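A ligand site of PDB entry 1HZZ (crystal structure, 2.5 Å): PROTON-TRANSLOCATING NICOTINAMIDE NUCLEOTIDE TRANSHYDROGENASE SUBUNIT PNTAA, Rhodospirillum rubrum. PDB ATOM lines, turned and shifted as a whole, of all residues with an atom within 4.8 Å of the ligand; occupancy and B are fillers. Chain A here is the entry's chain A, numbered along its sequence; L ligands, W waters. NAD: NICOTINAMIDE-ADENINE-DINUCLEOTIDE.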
ATOM      1  N   PRO A 126      27.081 -11.175  -7.203  1.00  0.00           N
ATOM      2  CA  PRO A 126      25.794 -10.927  -6.557  1.00  0.00           C
ATOM      3  C   PRO A 126      25.681 -11.719  -5.250  1.00  0.00           C
ATOM      4  O   PRO A 126      26.329 -12.742  -5.093  1.00  0.00           O
ATOM      5  CB  PRO A 126      24.792 -11.405  -7.595  1.00  0.00           C
ATOM      6  CG  PRO A 126      25.563 -12.455  -8.349  1.00  0.00           C
ATOM      7  CD  PRO A 126      26.892 -11.794  -8.530  1.00  0.00           C
ATOM      8  N   ARG A 127      24.871 -11.237  -4.313  1.00  0.00           N
ATOM      9  CA  ARG A 127      24.701 -11.928  -3.034  1.00  0.00           C
ATOM     10  C   ARG A 127      23.729 -13.101  -3.182  1.00  0.00           C
ATOM     11  O   ARG A 127      23.211 -13.612  -2.179  1.00  0.00           O
ATOM     12  CB  ARG A 127      24.178 -10.974  -1.948  1.00  0.00           C
ATOM     13  CG  ARG A 127      24.922  -9.646  -1.843  1.00  0.00           C
ATOM     14  CD  ARG A 127      26.340  -9.777  -1.314  1.00  0.00           C
ATOM     15  NE  ARG A 127      26.450  -9.516   0.118  1.00  0.00           N
ATOM     16  CZ  ARG A 127      27.608  -9.339   0.768  1.00  0.00           C
ATOM     17  NH1 ARG A 127      28.757  -9.384   0.114  1.00  0.00           N
ATOM     18  NH2 ARG A 127      27.602  -9.132   2.075  1.00  0.00           N
ATOM     19  N   ILE A 128      23.466 -13.531  -4.421  1.00  0.00           N
ATOM     20  CA  ILE A 128      22.561 -14.660  -4.604  1.00  0.00           C
ATOM     21  C   ILE A 128      23.211 -15.947  -4.086  1.00  0.00           C
ATOM     22  O   ILE A 128      24.433 -16.102  -4.148  1.00  0.00           O
ATOM     23  CB  ILE A 128      22.163 -14.851  -6.094  1.00  0.00           C
ATOM     24  CG1 ILE A 128      23.421 -14.926  -6.974  1.00  0.00           C
ATOM     25  CG2 ILE A 128      21.229 -13.731  -6.536  1.00  0.00           C
ATOM     26  CD1 ILE A 128      23.138 -15.397  -8.399  1.00  0.00           C
ATOM     27  N   SER A 129      22.395 -16.859  -3.577  1.00  0.00           N
ATOM     28  CA  SER A 129      22.919 -18.091  -2.999  1.00  0.00           C
ATOM     29  C   SER A 129      23.611 -19.085  -3.912  1.00  0.00           C
ATOM     30  O   SER A 129      24.522 -19.764  -3.466  1.00  0.00           O
ATOM     31  CB  SER A 129      21.823 -18.832  -2.246  1.00  0.00           C
ATOM     32  OG  SER A 129      22.362 -20.051  -1.757  1.00  0.00           O
ATOM     33  N   ALA A 131      25.703 -18.649  -5.660  1.00  0.00           N
ATOM     34  CA  ALA A 131      27.011 -18.032  -5.894  1.00  0.00           C
ATOM     35  C   ALA A 131      27.974 -18.172  -4.722  1.00  0.00           C
ATOM     36  O   ALA A 131      29.104 -17.707  -4.797  1.00  0.00           O
ATOM     37  CB  ALA A 131      26.834 -16.556  -6.235  1.00  0.00           C
ATOM     38  N   GLN A 132      27.533 -18.802  -3.624  1.00  0.00           N
ATOM     39  CA  GLN A 132      28.396 -18.990  -2.467  1.00  0.00           C
ATOM     40  C   GLN A 132      29.707 -19.574  -2.905  1.00  0.00           C
ATOM     41  O   GLN A 132      30.765 -19.120  -2.490  1.00  0.00           O
ATOM     42  CB  GLN A 132      27.782 -19.940  -1.452  1.00  0.00           C
ATOM     43  CG  GLN A 132      26.863 -19.284  -0.462  1.00  0.00           C
ATOM     44  CD  GLN A 132      27.404 -19.342   0.956  1.00  0.00           C
ATOM     45  OE1 GLN A 132      28.481 -18.803   1.256  1.00  0.00           O
ATOM     46  NE2 GLN A 132      26.647 -20.014   1.825  1.00  0.00           N
ATOM     47  N   ASP A 135      31.976 -16.832  -4.321  1.00  0.00           N
ATOM     48  CA  ASP A 135      32.287 -15.670  -3.508  1.00  0.00           C
ATOM     49  C   ASP A 135      33.706 -15.662  -2.955  1.00  0.00           C
ATOM     50  O   ASP A 135      34.018 -16.412  -2.027  1.00  0.00           O
ATOM     51  CB  ASP A 135      31.291 -15.605  -2.348  1.00  0.00           C
ATOM     52  CG  ASP A 135      30.799 -14.201  -2.089  1.00  0.00           C
ATOM     53  OD1 ASP A 135      31.585 -13.360  -1.618  1.00  0.00           O
ATOM     54  OD2 ASP A 135      29.603 -13.940  -2.366  1.00  0.00           O
ATOM     55  N   SER A 138      33.658 -14.179   0.864  1.00  0.00           N
ATOM     56  CA  SER A 138      33.404 -15.172   1.921  1.00  0.00           C
ATOM     57  C   SER A 138      34.542 -16.172   2.156  1.00  0.00           C
ATOM     58  O   SER A 138      34.981 -16.351   3.292  1.00  0.00           O
ATOM     59  CB  SER A 138      32.137 -15.951   1.592  1.00  0.00           C
ATOM     60  OG  SER A 138      31.132 -15.098   1.114  1.00  0.00           O
ATOM     61  N   GLY A 179      30.720  -7.303  14.924  1.00  0.00           N
ATOM     62  CA  GLY A 179      30.345  -7.628  13.555  1.00  0.00           C
ATOM     63  C   GLY A 179      30.350  -9.132  13.334  1.00  0.00           C
ATOM     64  O   GLY A 179      31.347  -9.698  12.862  1.00  0.00           O
ATOM     65  N   VAL A 180      29.229  -9.775  13.674  1.00  0.00           N
ATOM     66  CA  VAL A 180      29.098 -11.210  13.527  1.00  0.00           C
ATOM     67  C   VAL A 180      28.715 -11.632  12.106  1.00  0.00           C
ATOM     68  O   VAL A 180      27.632 -12.179  11.884  1.00  0.00           O
ATOM     69  CB  VAL A 180      28.033 -11.766  14.502  1.00  0.00           C
ATOM     70  CG1 VAL A 180      28.194 -13.259  14.661  1.00  0.00           C
ATOM     71  CG2 VAL A 180      28.162 -11.066  15.829  1.00  0.00           C
ATOM     72  N   GLY A 181      29.591 -11.352  11.149  1.00  0.00           N
ATOM     73  CA  GLY A 181      29.342 -11.738   9.765  1.00  0.00           C
ATOM     74  C   GLY A 181      30.120 -13.015   9.522  1.00  0.00           C
ATOM     75  O   GLY A 181      30.323 -13.787  10.468  1.00  0.00           O
ATOM     76  N   VAL A 182      30.591 -13.258   8.301  1.00  0.00           N
ATOM     77  CA  VAL A 182      31.336 -14.487   8.011  1.00  0.00           C
ATOM     78  C   VAL A 182      32.637 -14.575   8.802  1.00  0.00           C
ATOM     79  O   VAL A 182      32.951 -15.619   9.383  1.00  0.00           O
ATOM     80  CB  VAL A 182      31.709 -14.606   6.534  1.00  0.00           C
ATOM     81  CG1 VAL A 182      32.750 -15.701   6.359  1.00  0.00           C
ATOM     82  CG2 VAL A 182      30.483 -14.940   5.721  1.00  0.00           C
ATOM     83  N   ALA A 183      33.407 -13.480   8.793  1.00  0.00           N
ATOM     84  CA  ALA A 183      34.669 -13.428   9.502  1.00  0.00           C
ATOM     85  C   ALA A 183      34.399 -13.385  10.986  1.00  0.00           C
ATOM     86  O   ALA A 183      35.154 -13.946  11.779  1.00  0.00           O
ATOM     87  CB  ALA A 183      35.441 -12.215   9.089  1.00  0.00           C
ATOM     88  N   THR A 201      28.272  -8.804  19.031  1.00  0.00           N
ATOM     89  CA  THR A 201      27.234  -7.865  18.721  1.00  0.00           C
ATOM     90  C   THR A 201      27.264  -7.573  17.232  1.00  0.00           C
ATOM     91  O   THR A 201      28.315  -7.662  16.595  1.00  0.00           O
ATOM     92  CB  THR A 201      27.391  -6.557  19.498  1.00  0.00           C
ATOM     93  OG1 THR A 201      26.112  -5.895  19.544  1.00  0.00           O
ATOM     94  CG2 THR A 201      28.423  -5.636  18.827  1.00  0.00           C
ATOM     95  N   ASP A 202      26.080  -7.258  16.698  1.00  0.00           N
ATOM     96  CA  ASP A 202      25.892  -6.947  15.285  1.00  0.00           C
ATOM     97  C   ASP A 202      24.540  -6.227  15.216  1.00  0.00           C
ATOM     98  O   ASP A 202      23.680  -6.431  16.072  1.00  0.00           O
ATOM     99  CB  ASP A 202      25.824  -8.237  14.444  1.00  0.00           C
ATOM    100  CG  ASP A 202      26.199  -8.020  12.974  1.00  0.00           C
ATOM    101  OD1 ASP A 202      25.434  -7.361  12.218  1.00  0.00           O
ATOM    102  OD2 ASP A 202      27.271  -8.509  12.556  1.00  0.00           O
ATOM    103  N   VAL A 203      24.367  -5.401  14.191  1.00  0.00           N
ATOM    104  CA  VAL A 203      23.123  -4.676  14.003  1.00  0.00           C
ATOM    105  C   VAL A 203      22.023  -5.592  13.435  1.00  0.00           C
ATOM    106  O   VAL A 203      20.842  -5.394  13.720  1.00  0.00           O
ATOM    107  CB  VAL A 203      23.319  -3.477  13.052  1.00  0.00           C
ATOM    108  CG1 VAL A 203      23.963  -2.338  13.805  1.00  0.00           C
ATOM    109  CG2 VAL A 203      24.184  -3.874  11.877  1.00  0.00           C
ATOM    110  N   ARG A 204      22.420  -6.588  12.631  1.00  0.00           N
ATOM    111  CA  ARG A 204      21.473  -7.525  12.029  1.00  0.00           C
ATOM    112  C   ARG A 204      20.823  -8.469  13.045  1.00  0.00           C
ATOM    113  O   ARG A 204      21.500  -9.030  13.908  1.00  0.00           O
ATOM    114  CB  ARG A 204      22.158  -8.331  10.913  1.00  0.00           C
ATOM    115  CG  ARG A 204      22.752  -7.460   9.814  1.00  0.00           C
ATOM    116  CD  ARG A 204      22.988  -8.199   8.496  1.00  0.00           C
ATOM    117  NE  ARG A 204      24.219  -9.002   8.482  1.00  0.00           N
ATOM    118  CZ  ARG A 204      24.306 -10.256   8.939  1.00  0.00           C
ATOM    119  NH1 ARG A 204      23.243 -10.854   9.449  1.00  0.00           N
ATOM    120  NH2 ARG A 204      25.466 -10.894   8.891  1.00  0.00           N
ATOM    121  N   THR A 207      21.661 -12.560  13.172  1.00  0.00           N
ATOM    122  CA  THR A 207      22.933 -12.712  13.839  1.00  0.00           C
ATOM    123  C   THR A 207      22.845 -13.306  15.242  1.00  0.00           C
ATOM    124  O   THR A 207      23.534 -14.273  15.540  1.00  0.00           O
ATOM    125  CB  THR A 207      23.623 -11.355  13.910  1.00  0.00           C
ATOM    126  OG1 THR A 207      24.461 -11.196  12.761  1.00  0.00           O
ATOM    127  CG2 THR A 207      24.450 -11.239  15.153  1.00  0.00           C
ATOM    128  N   GLY A 234      21.508  -8.342   1.631  1.00  0.00           N
ATOM    129  CA  GLY A 234      22.520  -9.311   2.023  1.00  0.00           C
ATOM    130  C   GLY A 234      23.416  -8.792   3.141  1.00  0.00           C
ATOM    131  O   GLY A 234      24.296  -9.494   3.611  1.00  0.00           O
ATOM    132  N   ALA A 236      23.897  -4.787   5.839  1.00  0.00           N
ATOM    133  CA  ALA A 236      23.229  -3.713   6.564  1.00  0.00           C
ATOM    134  C   ALA A 236      23.665  -2.331   6.100  1.00  0.00           C
ATOM    135  O   ALA A 236      24.598  -2.193   5.319  1.00  0.00           O
ATOM    136  CB  ALA A 236      23.477  -3.847   8.055  1.00  0.00           C
ATOM    137  N   MET A 239      23.462   3.285  10.879  1.00  0.00           N
ATOM    138  CA  MET A 239      22.480   3.251  11.938  1.00  0.00           C
ATOM    139  C   MET A 239      22.295   4.639  12.511  1.00  0.00           C
ATOM    140  O   MET A 239      21.349   4.898  13.262  1.00  0.00           O
ATOM    141  CB  MET A 239      22.957   2.286  13.016  1.00  0.00           C
ATOM    142  CG  MET A 239      23.091   0.862  12.511  1.00  0.00           C
ATOM    143  SD  MET A 239      21.316   0.244  11.758  1.00  0.00           S
ATOM    144  CE  MET A 239      20.791  -1.141  13.130  1.00  0.00           C
ATOM    145  N   PHE A 243      22.247   5.794  17.151  1.00  0.00           N
ATOM    146  CA  PHE A 243      22.379   4.354  17.393  1.00  0.00           C
ATOM    147  C   PHE A 243      23.776   4.049  17.906  1.00  0.00           C
ATOM    148  O   PHE A 243      23.947   3.405  18.949  1.00  0.00           O
ATOM    149  CB  PHE A 243      22.147   3.564  16.099  1.00  0.00           C
ATOM    150  CG  PHE A 243      22.325   2.083  16.268  1.00  0.00           C
ATOM    151  CD1 PHE A 243      21.305   1.299  16.782  1.00  0.00           C
ATOM    152  CD2 PHE A 243      23.525   1.475  15.901  1.00  0.00           C
ATOM    153  CE1 PHE A 243      21.482  -0.076  16.932  1.00  0.00           C
ATOM    154  CE2 PHE A 243      23.709   0.108  16.051  1.00  0.00           C
ATOM    155  CZ  PHE A 243      22.689  -0.676  16.564  1.00  0.00           C
ATOM    156  N   GLN A 247      24.739   2.032  21.155  1.00  0.00           N
ATOM    157  CA  GLN A 247      25.598   0.842  21.051  1.00  0.00           C
ATOM    158  C   GLN A 247      26.742   0.915  22.042  1.00  0.00           C
ATOM    159  O   GLN A 247      26.778   0.163  23.019  1.00  0.00           O
ATOM    160  CB  GLN A 247      26.177   0.712  19.636  1.00  0.00           C
ATOM    161  CG  GLN A 247      26.713  -0.672  19.325  1.00  0.00           C
ATOM    162  CD  GLN A 247      27.149  -0.829  17.878  1.00  0.00           C
ATOM    163  OE1 GLN A 247      27.210  -1.938  17.335  1.00  0.00           O
ATOM    164  NE2 GLN A 247      27.465   0.292  17.244  1.00  0.00           N
ATOM    165  N   THR A 264      34.984  -6.317  12.800  1.00  0.00           N
ATOM    166  CA  THR A 264      34.903  -6.785  11.419  1.00  0.00           C
ATOM    167  C   THR A 264      33.796  -6.102  10.611  1.00  0.00           C
ATOM    168  O   THR A 264      33.596  -6.415   9.429  1.00  0.00           O
ATOM    169  CB  THR A 264      34.640  -8.315  11.377  1.00  0.00           C
ATOM    170  OG1 THR A 264      33.416  -8.603  12.063  1.00  0.00           O
ATOM    171  CG2 THR A 264      35.765  -9.077  12.055  1.00  0.00           C
ATOM    172  N   ALA A 265      33.075  -5.171  11.247  1.00  0.00           N
ATOM    173  CA  ALA A 265      31.978  -4.472  10.577  1.00  0.00           C
ATOM    174  C   ALA A 265      32.435  -3.779   9.307  1.00  0.00           C
ATOM    175  O   ALA A 265      33.533  -3.230   9.237  1.00  0.00           O
ATOM    176  CB  ALA A 265      31.352  -3.477  11.526  1.00  0.00           C
ATOM    177  N   LEU A 266      31.582  -3.790   8.302  1.00  0.00           N
ATOM    178  CA  LEU A 266      31.904  -3.166   7.028  1.00  0.00           C
ATOM    179  C   LEU A 266      30.591  -2.702   6.387  1.00  0.00           C
ATOM    180  O   LEU A 266      29.526  -3.217   6.735  1.00  0.00           O
ATOM    181  CB  LEU A 266      32.582  -4.197   6.136  1.00  0.00           C
ATOM    182  CG  LEU A 266      33.866  -3.776   5.436  1.00  0.00           C
ATOM    183  CD1 LEU A 266      34.841  -3.199   6.440  1.00  0.00           C
ATOM    184  CD2 LEU A 266      34.464  -4.984   4.745  1.00  0.00           C
ATOM    185  N   ILE A 267      30.664  -1.737   5.474  1.00  0.00           N
ATOM    186  CA  ILE A 267      29.449  -1.229   4.817  1.00  0.00           C
ATOM    187  C   ILE A 267      29.621  -0.945   3.309  1.00  0.00           C
ATOM    188  O   ILE A 267      30.247   0.038   2.928  1.00  0.00           O
ATOM    189  CB  ILE A 267      28.937   0.052   5.510  1.00  0.00           C
ATOM    190  CG1 ILE A 267      28.513  -0.293   6.930  1.00  0.00           C
ATOM    191  CG2 ILE A 267      27.785   0.634   4.741  1.00  0.00           C
ATOM    192  CD1 ILE A 267      27.917   0.870   7.682  1.00  0.00           C
ATOM    193  N   PRO A 273      32.273   1.438   9.640  1.00  0.00           N
ATOM    194  CA  PRO A 273      31.612   2.077  10.770  1.00  0.00           C
ATOM    195  C   PRO A 273      32.468   2.103  12.031  1.00  0.00           C
ATOM    196  O   PRO A 273      33.041   1.083  12.442  1.00  0.00           O
ATOM    197  CB  PRO A 273      30.349   1.235  10.945  1.00  0.00           C
ATOM    198  CG  PRO A 273      30.805  -0.111  10.526  1.00  0.00           C
ATOM    199  CD  PRO A 273      31.581   0.192   9.265  1.00  0.00           C
ATOM    200  N   LEU A 275      33.454   1.744  15.603  1.00  0.00           N
ATOM    201  CA  LEU A 275      32.975   0.901  16.685  1.00  0.00           C
ATOM    202  C   LEU A 275      33.724   1.048  18.018  1.00  0.00           C
ATOM    203  O   LEU A 275      33.142   0.821  19.075  1.00  0.00           O
ATOM    204  CB  LEU A 275      33.028  -0.561  16.251  1.00  0.00           C
ATOM    205  CG  LEU A 275      32.132  -0.940  15.081  1.00  0.00           C
ATOM    206  CD1 LEU A 275      32.717  -2.140  14.374  1.00  0.00           C
ATOM    207  CD2 LEU A 275      30.731  -1.236  15.589  1.00  0.00           C
HETATM  208  PA  NAD L   1      30.411  -7.808   5.794  1.00  0.00           P
HETATM  209  O1A NAD L   1      31.813  -8.342   5.946  1.00  0.00           O
HETATM  210  O2A NAD L   1      30.363  -6.608   4.919  1.00  0.00           O
HETATM  211  O5B NAD L   1      29.747  -7.452   7.214  1.00  0.00           O
HETATM  212  C5B NAD L   1      30.428  -7.597   8.467  1.00  0.00           C
HETATM  213  C4B NAD L   1      29.431  -7.379   9.571  1.00  0.00           C
HETATM  214  O4B NAD L   1      29.389  -5.955   9.846  1.00  0.00           O
HETATM  215  C3B NAD L   1      27.937  -7.705   9.283  1.00  0.00           C
HETATM  216  O3B NAD L   1      27.371  -8.729  10.043  1.00  0.00           O
HETATM  217  C2B NAD L   1      27.245  -6.380   9.462  1.00  0.00           C
HETATM  218  O2B NAD L   1      25.873  -6.459   9.742  1.00  0.00           O
HETATM  219  C1B NAD L   1      28.155  -5.787  10.533  1.00  0.00           C
HETATM  220  N9A NAD L   1      28.027  -4.307  10.845  1.00  0.00           N
HETATM  221  C8A NAD L   1      28.158  -3.207  10.004  1.00  0.00           C
HETATM  222  N7A NAD L   1      27.998  -2.019  10.647  1.00  0.00           N
HETATM  223  C5A NAD L   1      27.750  -2.392  11.953  1.00  0.00           C
HETATM  224  C6A NAD L   1      27.475  -1.638  13.159  1.00  0.00           C
HETATM  225  N6A NAD L   1      27.418  -0.307  13.215  1.00  0.00           N
HETATM  226  N1A NAD L   1      27.257  -2.367  14.365  1.00  0.00           N
HETATM  227  C2A NAD L   1      27.314  -3.770  14.358  1.00  0.00           C
HETATM  228  N3A NAD L   1      27.557  -4.527  13.288  1.00  0.00           N
HETATM  229  C4A NAD L   1      27.765  -3.798  12.102  1.00  0.00           C
HETATM  230  O3  NAD L   1      29.332  -8.946   5.456  1.00  0.00           O
HETATM  231  PN  NAD L   1      29.510 -10.453   5.242  1.00  0.00           P
HETATM  232  O1N NAD L   1      30.139 -11.071   6.453  1.00  0.00           O
HETATM  233  O2N NAD L   1      30.392 -10.690   4.065  1.00  0.00           O
HETATM  234  O5D NAD L   1      28.186 -11.057   4.998  1.00  0.00           O
HETATM  235  C5D NAD L   1      27.081 -11.035   5.824  1.00  0.00           C
HETATM  236  C4D NAD L   1      25.961 -11.594   5.576  1.00  0.00           C
HETATM  237  O4D NAD L   1      25.815 -11.638   4.120  1.00  0.00           O
HETATM  238  C3D NAD L   1      26.063 -13.024   6.102  1.00  0.00           C
HETATM  239  O3D NAD L   1      24.866 -13.345   6.817  1.00  0.00           O
HETATM  240  C2D NAD L   1      26.319 -13.858   4.813  1.00  0.00           C
HETATM  241  O2D NAD L   1      25.841 -14.876   4.750  1.00  0.00           O
HETATM  242  C1D NAD L   1      25.797 -13.014   3.661  1.00  0.00           C
HETATM  243  N1N NAD L   1      26.527 -13.165   2.429  1.00  0.00           N
HETATM  244  C2N NAD L   1      26.020 -14.091   1.507  1.00  0.00           C
HETATM  245  C3N NAD L   1      26.696 -14.288   0.280  1.00  0.00           C
HETATM  246  C7N NAD L   1      26.330 -15.278  -0.903  1.00  0.00           C
HETATM  247  O7N NAD L   1      26.036 -16.456  -0.637  1.00  0.00           O
HETATM  248  N7N NAD L   1      26.338 -14.788  -2.154  1.00  0.00           N
HETATM  249  C4N NAD L   1      27.921 -13.529  -0.026  1.00  0.00           C
HETATM  250  C5N NAD L   1      28.375 -12.600   0.950  1.00  0.00           C
HETATM  251  C6N NAD L   1      27.764 -12.352   2.182  1.00  0.00           C
HETATM  252  O   HOH W   1      26.080 -13.775   9.605  1.00  0.00           O
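O4B of the ligand is in hydrogen-bond range of N of Leu 266 (3.4 Å). An oxygen (O1N) of the ligand is in hydrogen-bond range of the backbone NH (N) of Val 182. NH2 of Arg 127 is in salt-bridge range of O2N of the ligand. A nitrogen (N7N) of the ligand sits close to the side-chain carboxylate (OD2) of Asp 135, 3.4 Å away. The side-chain amide oxygen of Gln 247 sits close to a nitrogen (N1A) of the ligand, 3.0 Å away. A nitrogen (N7N) of the ligand lies close to the backbone carbonyl oxygen of Arg 127. An oxygen (O3B) of the ligand lies within hydrogen-bond range of the guanidinium group (NH2) of Arg 204 (3.1 Å). The backbone carbonyl oxygen of Gly 234 lies close to an oxygen (O4D) of the ligand. The backbone carbonyl oxygen of Ile 128 is in hydrogen-bond range of a nitrogen (N7N) of the ligand (3.1 Å). An oxygen (O3B) of the ligand lies within hydrogen-bond range of the side-chain carboxylate (OD2) of Asp 202 (2.5 Å). A nitrogen (N3A) of the ligand sits close to the backbone NH (N) of Val 203 (3.4 Å).
The side-chain carboxylate (OD1) of Asp 135 is in hydrogen-bond range of the side-chain hydroxyl (OG) of Ser 138 (3.3 Å). The side-chain hydroxyl (OG1) of Thr 207 sits at hydrogen-bond distance from the backbone carbonyl oxygen (O) of Val 180, 3.4 Å away. The backbone NH (N) of Val 180 is in hydrogen-bond range of the side-chain carboxylate (OD2) of Asp 202. OD1 of Asp 202 sits at hydrogen-bond distance from N of Arg 204 (3.1 Å). OG1 of Thr 264 lies within hydrogen-bond range of O of Gly 179.
Merely in contact with the ligand: Gln 132, Ala 265, Pro 273, Gly 181, Thr 264, Pro 126, Ser 138, Val 180, Leu 275 and Ala 236. Hydrophobic or aromatic side chains that line the ligand: Val 182, Val 203, Ala 236, Ala 265, Leu 266, Pro 273 and Leu 275. 20 residues have an atom within 4 Å of the ligand: Pro 126, Arg 127, Ile 128, Gln 132, Asp 135, Ser 138, Val 180, Gly 181, Val 182, Asp 202, Val 203, Arg 204, Gly 234, Ala 236, Gln 247, Thr 264, Ala 265, Leu 266, Pro 273 and Leu 275. Along chain A the residues within 4 Å of the ligand span positions 126 to 275. The nearest printed residue that does not touch the ligand is Gly 179 (4.1 Å).
Water W1 lies within hydrogen-bond range of NH2 of Arg 204, O3D of the ligand and O of Val 180.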
